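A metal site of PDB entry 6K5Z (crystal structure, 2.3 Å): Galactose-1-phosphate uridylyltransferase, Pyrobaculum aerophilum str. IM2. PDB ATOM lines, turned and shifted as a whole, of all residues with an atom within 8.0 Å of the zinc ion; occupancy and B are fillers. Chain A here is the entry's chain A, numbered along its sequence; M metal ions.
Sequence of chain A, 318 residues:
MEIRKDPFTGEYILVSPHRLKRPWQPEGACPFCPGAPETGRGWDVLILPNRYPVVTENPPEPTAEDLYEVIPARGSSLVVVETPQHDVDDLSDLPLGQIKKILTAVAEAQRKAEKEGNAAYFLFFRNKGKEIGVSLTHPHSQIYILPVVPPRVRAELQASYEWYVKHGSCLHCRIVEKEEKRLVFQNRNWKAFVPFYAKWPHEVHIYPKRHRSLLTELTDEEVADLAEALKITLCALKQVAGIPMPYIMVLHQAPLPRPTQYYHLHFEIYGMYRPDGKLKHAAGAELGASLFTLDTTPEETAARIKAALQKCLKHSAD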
ATOM      1  N   TYR A 164     -31.410  10.379 -18.729  1.00  0.00           N
ATOM      2  CA  TYR A 164     -30.901  10.766 -17.430  1.00  0.00           C
ATOM      3  C   TYR A 164     -31.944  11.543 -16.643  1.00  0.00           C
ATOM      4  O   TYR A 164     -32.229  11.220 -15.486  1.00  0.00           O
ATOM      5  CB  TYR A 164     -29.638  11.613 -17.574  1.00  0.00           C
ATOM      6  CG  TYR A 164     -28.976  11.883 -16.251  1.00  0.00           C
ATOM      7  CD1 TYR A 164     -28.292  10.874 -15.595  1.00  0.00           C
ATOM      8  CD2 TYR A 164     -29.040  13.133 -15.628  1.00  0.00           C
ATOM      9  CE1 TYR A 164     -27.671  11.074 -14.375  1.00  0.00           C
ATOM     10  CE2 TYR A 164     -28.419  13.360 -14.397  1.00  0.00           C
ATOM     11  CZ  TYR A 164     -27.735  12.318 -13.772  1.00  0.00           C
ATOM     12  OH  TYR A 164     -27.105  12.493 -12.545  1.00  0.00           O
ATOM     13  N   SER A 169     -30.303   8.466 -13.598  1.00  0.00           N
ATOM     14  CA  SER A 169     -28.986   7.831 -13.698  1.00  0.00           C
ATOM     15  C   SER A 169     -28.478   7.697 -15.136  1.00  0.00           C
ATOM     16  O   SER A 169     -29.236   7.864 -16.111  1.00  0.00           O
ATOM     17  CB  SER A 169     -29.055   6.461 -13.081  1.00  0.00           C
ATOM     18  OG  SER A 169     -29.682   5.580 -13.988  1.00  0.00           O
ATOM     19  N   CYS A 170     -27.185   7.402 -15.268  1.00  0.00           N
ATOM     20  CA  CYS A 170     -26.540   7.170 -16.572  1.00  0.00           C
ATOM     21  C   CYS A 170     -26.982   5.851 -17.233  1.00  0.00           C
ATOM     22  O   CYS A 170     -26.831   4.749 -16.668  1.00  0.00           O
ATOM     23  CB  CYS A 170     -25.009   7.173 -16.441  1.00  0.00           C
ATOM     24  SG  CYS A 170     -24.166   6.854 -18.035  1.00  0.00           S
ATOM     25  N   LEU A 171     -27.507   5.952 -18.450  1.00  0.00           N
ATOM     26  CA  LEU A 171     -28.057   4.788 -19.167  1.00  0.00           C
ATOM     27  C   LEU A 171     -26.928   3.828 -19.501  1.00  0.00           C
ATOM     28  O   LEU A 171     -27.072   2.607 -19.389  1.00  0.00           O
ATOM     29  CB  LEU A 171     -28.777   5.210 -20.460  1.00  0.00           C
ATOM     30  CG  LEU A 171     -29.326   4.082 -21.397  1.00  0.00           C
ATOM     31  CD1 LEU A 171     -30.147   3.076 -20.622  1.00  0.00           C
ATOM     32  CD2 LEU A 171     -30.178   4.617 -22.545  1.00  0.00           C
ATOM     33  N   HIS A 172     -25.786   4.404 -19.855  1.00  0.00           N
ATOM     34  CA  HIS A 172     -24.573   3.657 -20.151  1.00  0.00           C
ATOM     35  C   HIS A 172     -24.054   2.909 -18.924  1.00  0.00           C
ATOM     36  O   HIS A 172     -23.672   1.748 -19.033  1.00  0.00           O
ATOM     37  CB  HIS A 172     -23.470   4.584 -20.642  1.00  0.00           C
ATOM     38  CG  HIS A 172     -23.851   5.398 -21.839  1.00  0.00           C
ATOM     39  ND1 HIS A 172     -23.550   5.009 -23.124  1.00  0.00           N
ATOM     40  CD2 HIS A 172     -24.495   6.581 -21.942  1.00  0.00           C
ATOM     41  CE1 HIS A 172     -23.999   5.920 -23.972  1.00  0.00           C
ATOM     42  NE2 HIS A 172     -24.574   6.883 -23.278  1.00  0.00           N
ATOM     43  N   CYS A 173     -24.036   3.562 -17.764  1.00  0.00           N
ATOM     44  CA  CYS A 173     -23.571   2.907 -16.554  1.00  0.00           C
ATOM     45  C   CYS A 173     -24.486   1.730 -16.260  1.00  0.00           C
ATOM     46  O   CYS A 173     -24.041   0.661 -15.855  1.00  0.00           O
ATOM     47  CB  CYS A 173     -23.537   3.904 -15.385  1.00  0.00           C
ATOM     48  SG  CYS A 173     -21.934   4.700 -15.172  1.00  0.00           S
ATOM     49  N   ARG A 174     -25.783   1.946 -16.460  1.00  0.00           N
ATOM     50  CA  ARG A 174     -26.785   0.907 -16.281  1.00  0.00           C
ATOM     51  C   ARG A 174     -26.624  -0.243 -17.280  1.00  0.00           C
ATOM     52  O   ARG A 174     -26.773  -1.407 -16.924  1.00  0.00           O
ATOM     53  CB  ARG A 174     -28.194   1.489 -16.351  1.00  0.00           C
ATOM     54  CG  ARG A 174     -29.278   0.563 -15.828  1.00  0.00           C
ATOM     55  CD  ARG A 174     -30.577   1.303 -15.582  1.00  0.00           C
ATOM     56  NE  ARG A 174     -31.594   0.441 -15.006  1.00  0.00           N
ATOM     57  CZ  ARG A 174     -32.795   0.866 -14.602  1.00  0.00           C
ATOM     58  NH1 ARG A 174     -33.126   2.142 -14.716  1.00  0.00           N
ATOM     59  NH2 ARG A 174     -33.669   0.003 -14.090  1.00  0.00           N
ATOM     60  N   ILE A 175     -26.309   0.093 -18.536  1.00  0.00           N
ATOM     61  CA  ILE A 175     -26.167  -0.923 -19.586  1.00  0.00           C
ATOM     62  C   ILE A 175     -24.973  -1.838 -19.329  1.00  0.00           C
ATOM     63  O   ILE A 175     -25.056  -3.051 -19.470  1.00  0.00           O
ATOM     64  CB  ILE A 175     -25.994  -0.287 -20.973  1.00  0.00           C
ATOM     65  CG1 ILE A 175     -27.300   0.320 -21.471  1.00  0.00           C
ATOM     66  CG2 ILE A 175     -25.480  -1.325 -21.969  1.00  0.00           C
ATOM     67  CD1 ILE A 175     -27.180   1.026 -22.795  1.00  0.00           C
ATOM     68  N   VAL A 176     -23.854  -1.221 -18.952  1.00  0.00           N
ATOM     69  CA  VAL A 176     -22.634  -1.919 -18.625  1.00  0.00           C
ATOM     70  C   VAL A 176     -22.789  -2.904 -17.435  1.00  0.00           C
ATOM     71  O   VAL A 176     -22.211  -3.985 -17.487  1.00  0.00           O
ATOM     72  CB  VAL A 176     -21.479  -0.907 -18.380  1.00  0.00           C
ATOM     73  CG1 VAL A 176     -20.187  -1.613 -17.957  1.00  0.00           C
ATOM     74  CG2 VAL A 176     -21.190  -0.100 -19.622  1.00  0.00           C
ATOM     75  N   GLU A 177     -23.568  -2.544 -16.429  1.00  0.00           N
ATOM     76  CA  GLU A 177     -23.751  -3.410 -15.275  1.00  0.00           C
ATOM     77  C   GLU A 177     -24.427  -4.722 -15.663  1.00  0.00           C
ATOM     78  O   GLU A 177     -24.053  -5.777 -15.177  1.00  0.00           O
ATOM     79  CB  GLU A 177     -24.619  -2.728 -14.209  1.00  0.00           C
ATOM     80  CG  GLU A 177     -24.249  -1.281 -13.891  1.00  0.00           C
ATOM     81  CD  GLU A 177     -25.313  -0.584 -13.058  1.00  0.00           C
ATOM     82  OE1 GLU A 177     -26.284  -1.253 -12.647  1.00  0.00           O
ATOM     83  OE2 GLU A 177     -25.179   0.627 -12.802  1.00  0.00           O
ATOM     84  N   TYR A 207     -16.257  -0.123 -22.871  1.00  0.00           N
ATOM     85  CA  TYR A 207     -16.708   0.901 -21.892  1.00  0.00           C
ATOM     86  C   TYR A 207     -15.880   0.815 -20.651  1.00  0.00           C
ATOM     87  O   TYR A 207     -15.524  -0.295 -20.222  1.00  0.00           O
ATOM     88  CB  TYR A 207     -18.120   0.602 -21.464  1.00  0.00           C
ATOM     89  CG  TYR A 207     -19.166   1.270 -22.275  1.00  0.00           C
ATOM     90  CD1 TYR A 207     -19.582   2.537 -21.957  1.00  0.00           C
ATOM     91  CD2 TYR A 207     -19.786   0.603 -23.310  1.00  0.00           C
ATOM     92  CE1 TYR A 207     -20.577   3.146 -22.688  1.00  0.00           C
ATOM     93  CE2 TYR A 207     -20.769   1.205 -24.080  1.00  0.00           C
ATOM     94  CZ  TYR A 207     -21.167   2.463 -23.760  1.00  0.00           C
ATOM     95  OH  TYR A 207     -22.131   3.050 -24.474  1.00  0.00           O
ATOM     96  N   PRO A 208     -15.571   1.956 -20.029  1.00  0.00           N
ATOM     97  CA  PRO A 208     -14.930   1.897 -18.710  1.00  0.00           C
ATOM     98  C   PRO A 208     -15.954   1.570 -17.618  1.00  0.00           C
ATOM     99  O   PRO A 208     -17.098   2.006 -17.688  1.00  0.00           O
ATOM    100  CB  PRO A 208     -14.391   3.306 -18.539  1.00  0.00           C
ATOM    101  CG  PRO A 208     -15.286   4.158 -19.334  1.00  0.00           C
ATOM    102  CD  PRO A 208     -15.862   3.328 -20.445  1.00  0.00           C
ATOM    103  N   LYS A 209     -15.535   0.802 -16.625  1.00  0.00           N
ATOM    104  CA  LYS A 209     -16.397   0.415 -15.537  1.00  0.00           C
ATOM    105  C   LYS A 209     -16.726   1.612 -14.697  1.00  0.00           C
ATOM    106  O   LYS A 209     -17.872   1.772 -14.306  1.00  0.00           O
ATOM    107  CB  LYS A 209     -15.768  -0.708 -14.699  1.00  0.00           C
ATOM    108  CG  LYS A 209     -15.874  -2.082 -15.324  1.00  0.00           C
ATOM    109  CD  LYS A 209     -15.138  -3.148 -14.504  1.00  0.00           C
ATOM    110  CE  LYS A 209     -15.418  -4.531 -15.104  1.00  0.00           C
ATOM    111  NZ  LYS A 209     -14.583  -5.653 -14.561  1.00  0.00           N
ATOM    112  N   ARG A 210     -15.753   2.458 -14.420  1.00  0.00           N
ATOM    113  CA  ARG A 210     -16.035   3.712 -13.734  1.00  0.00           C
ATOM    114  C   ARG A 210     -16.719   4.622 -14.747  1.00  0.00           C
ATOM    115  O   ARG A 210     -16.374   4.591 -15.933  1.00  0.00           O
ATOM    116  CB  ARG A 210     -14.759   4.386 -13.250  1.00  0.00           C
ATOM    117  CG  ARG A 210     -14.227   3.885 -11.921  1.00  0.00           C
ATOM    118  CD  ARG A 210     -13.141   4.820 -11.432  1.00  0.00           C
ATOM    119  NE  ARG A 210     -12.409   4.286 -10.293  1.00  0.00           N
ATOM    120  CZ  ARG A 210     -11.169   4.647  -9.976  1.00  0.00           C
ATOM    121  NH1 ARG A 210     -10.538   5.541 -10.714  1.00  0.00           N
ATOM    122  NH2 ARG A 210     -10.563   4.100  -8.936  1.00  0.00           N
ATOM    123  N   HIS A 211     -17.640   5.463 -14.305  1.00  0.00           N
ATOM    124  CA  HIS A 211     -18.296   6.356 -15.251  1.00  0.00           C
ATOM    125  C   HIS A 211     -17.296   7.426 -15.638  1.00  0.00           C
ATOM    126  O   HIS A 211     -16.799   8.154 -14.799  1.00  0.00           O
ATOM    127  CB  HIS A 211     -19.527   6.998 -14.609  1.00  0.00           C
ATOM    128  CG  HIS A 211     -20.084   8.144 -15.403  1.00  0.00           C
ATOM    129  ND1 HIS A 211     -21.175   8.004 -16.228  1.00  0.00           N
ATOM    130  CD2 HIS A 211     -19.699   9.433 -15.496  1.00  0.00           C
ATOM    131  CE1 HIS A 211     -21.443   9.167 -16.790  1.00  0.00           C
ATOM    132  NE2 HIS A 211     -20.563  10.048 -16.366  1.00  0.00           N
ATOM    133  N   ARG A 212     -17.016   7.508 -16.942  1.00  0.00           N
ATOM    134  CA  ARG A 212     -16.075   8.481 -17.477  1.00  0.00           C
ATOM    135  C   ARG A 212     -16.665   9.068 -18.738  1.00  0.00           C
ATOM    136  O   ARG A 212     -17.305   8.363 -19.510  1.00  0.00           O
ATOM    137  CB  ARG A 212     -14.742   7.815 -17.799  1.00  0.00           C
ATOM    138  CG  ARG A 212     -14.058   7.141 -16.627  1.00  0.00           C
ATOM    139  CD  ARG A 212     -13.672   8.149 -15.558  1.00  0.00           C
ATOM    140  NE  ARG A 212     -12.538   7.685 -14.768  1.00  0.00           N
ATOM    141  CZ  ARG A 212     -12.012   8.359 -13.756  1.00  0.00           C
ATOM    142  NH1 ARG A 212     -12.525   9.525 -13.396  1.00  0.00           N
ATOM    143  NH2 ARG A 212     -10.973   7.869 -13.093  1.00  0.00           N
ATOM    144  N   SER A 213     -16.434  10.345 -18.973  1.00  0.00           N
ATOM    145  CA  SER A 213     -16.975  11.010 -20.164  1.00  0.00           C
ATOM    146  C   SER A 213     -15.942  11.498 -21.096  1.00  0.00           C
ATOM    147  O   SER A 213     -16.256  11.762 -22.229  1.00  0.00           O
ATOM    148  CB  SER A 213     -17.885  12.170 -19.767  1.00  0.00           C
ATOM    149  OG  SER A 213     -17.293  12.978 -18.775  1.00  0.00           O
ATOM    150  N   THR A 260     -19.426  15.069 -18.368  1.00  0.00           N
ATOM    151  CA  THR A 260     -20.883  14.917 -18.329  1.00  0.00           C
ATOM    152  C   THR A 260     -21.313  13.780 -17.445  1.00  0.00           C
ATOM    153  O   THR A 260     -20.762  12.676 -17.542  1.00  0.00           O
ATOM    154  CB  THR A 260     -21.486  14.565 -19.711  1.00  0.00           C
ATOM    155  OG1 THR A 260     -21.080  13.231 -20.113  1.00  0.00           O
ATOM    156  CG2 THR A 260     -21.133  15.632 -20.761  1.00  0.00           C
ATOM    157  N   GLN A 261     -22.352  14.024 -16.642  1.00  0.00           N
ATOM    158  CA  GLN A 261     -22.850  12.975 -15.774  1.00  0.00           C
ATOM    159  C   GLN A 261     -23.783  12.007 -16.526  1.00  0.00           C
ATOM    160  O   GLN A 261     -23.937  10.876 -16.106  1.00  0.00           O
ATOM    161  CB  GLN A 261     -23.506  13.574 -14.508  1.00  0.00           C
ATOM    162  CG  GLN A 261     -24.886  14.209 -14.699  1.00  0.00           C
ATOM    163  CD  GLN A 261     -25.435  14.892 -13.438  1.00  0.00           C
ATOM    164  OE1 GLN A 261     -24.996  14.606 -12.320  1.00  0.00           O
ATOM    165  NE2 GLN A 261     -26.404  15.783 -13.628  1.00  0.00           N
ATOM    166  N   TYR A 262     -24.362  12.445 -17.647  1.00  0.00           N
ATOM    167  CA  TYR A 262     -25.332  11.672 -18.437  1.00  0.00           C
ATOM    168  C   TYR A 262     -24.719  10.885 -19.625  1.00  0.00           C
ATOM    169  O   TYR A 262     -25.386  10.012 -20.199  1.00  0.00           O
ATOM    170  CB  TYR A 262     -26.427  12.611 -19.017  1.00  0.00           C
ATOM    171  CG  TYR A 262     -25.897  13.790 -19.831  1.00  0.00           C
ATOM    172  CD1 TYR A 262     -25.567  14.980 -19.204  1.00  0.00           C
ATOM    173  CD2 TYR A 262     -25.769  13.735 -21.227  1.00  0.00           C
ATOM    174  CE1 TYR A 262     -25.094  16.073 -19.897  1.00  0.00           C
ATOM    175  CE2 TYR A 262     -25.288  14.839 -21.944  1.00  0.00           C
ATOM    176  CZ  TYR A 262     -24.952  16.007 -21.269  1.00  0.00           C
ATOM    177  OH  TYR A 262     -24.479  17.141 -21.901  1.00  0.00           O
ATOM    178  N   TYR A 263     -23.491  11.250 -20.030  1.00  0.00           N
ATOM    179  CA  TYR A 263     -22.792  10.558 -21.111  1.00  0.00           C
ATOM    180  C   TYR A 263     -21.535   9.905 -20.579  1.00  0.00           C
ATOM    181  O   TYR A 263     -20.892  10.382 -19.633  1.00  0.00           O
ATOM    182  CB  TYR A 263     -22.458  11.507 -22.272  1.00  0.00           C
ATOM    183  CG  TYR A 263     -22.151  10.817 -23.580  1.00  0.00           C
ATOM    184  CD1 TYR A 263     -23.087  10.003 -24.181  1.00  0.00           C
ATOM    185  CD2 TYR A 263     -20.938  11.010 -24.225  1.00  0.00           C
ATOM    186  CE1 TYR A 263     -22.833   9.394 -25.388  1.00  0.00           C
ATOM    187  CE2 TYR A 263     -20.643  10.369 -25.434  1.00  0.00           C
ATOM    188  CZ  TYR A 263     -21.598   9.569 -26.017  1.00  0.00           C
ATOM    189  OH  TYR A 263     -21.366   8.939 -27.218  1.00  0.00           O
ATOM    190  N   HIS A 264     -21.168   8.816 -21.233  1.00  0.00           N
ATOM    191  CA  HIS A 264     -20.195   7.886 -20.708  1.00  0.00           C
ATOM    192  C   HIS A 264     -19.401   7.411 -21.908  1.00  0.00           C
ATOM    193  O   HIS A 264     -19.957   6.795 -22.823  1.00  0.00           O
ATOM    194  CB  HIS A 264     -20.963   6.762 -20.002  1.00  0.00           C
ATOM    195  CG  HIS A 264     -20.126   5.700 -19.341  1.00  0.00           C
ATOM    196  ND1 HIS A 264     -20.557   5.010 -18.217  1.00  0.00           N
ATOM    197  CD2 HIS A 264     -18.937   5.151 -19.676  1.00  0.00           C
ATOM    198  CE1 HIS A 264     -19.667   4.108 -17.888  1.00  0.00           C
ATOM    199  NE2 HIS A 264     -18.666   4.168 -18.751  1.00  0.00           N
ATOM    200  N   LEU A 265     -18.105   7.705 -21.905  1.00  0.00           N
ATOM    201  CA  LEU A 265     -17.289   7.436 -23.044  1.00  0.00           C
ATOM    202  C   LEU A 265     -17.177   5.938 -23.404  1.00  0.00           C
ATOM    203  O   LEU A 265     -17.152   5.064 -22.499  1.00  0.00           O
ATOM    204  CB  LEU A 265     -15.887   8.054 -22.869  1.00  0.00           C
ATOM    205  CG  LEU A 265     -14.818   7.340 -22.055  1.00  0.00           C
ATOM    206  CD1 LEU A 265     -14.050   6.246 -22.815  1.00  0.00           C
ATOM    207  CD2 LEU A 265     -13.848   8.391 -21.537  1.00  0.00           C
HETATM  208 ZN    ZN M   1     -22.129   6.260 -16.963  1.00  0.00          ZN
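The zinc ion is bound by ND1 of His 211, ND1 of His 264, SG of Cys 170 and SG of Cys 173. The zinc ion has four donor atoms within binding distance.
The backbone carbonyl oxygen (O) of Gln 261 lies close to a ring nitrogen (NE2) of His 211, at 3.5 Å. A ring nitrogen (NE2) of His 211 sits close to the backbone carbonyl oxygen of Tyr 263 (3.3 Å). A ring nitrogen (NE2) of His 211 lies within hydrogen-bond range of the backbone carbonyl oxygen of Thr 260, 2.9 Å away. A ring nitrogen (NE2) of His 264 lies within hydrogen-bond range of the backbone carbonyl oxygen (O) of Pro 208 (2.9 Å). SG of Cys 170 lies close to N of His 172 (3.5 Å).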
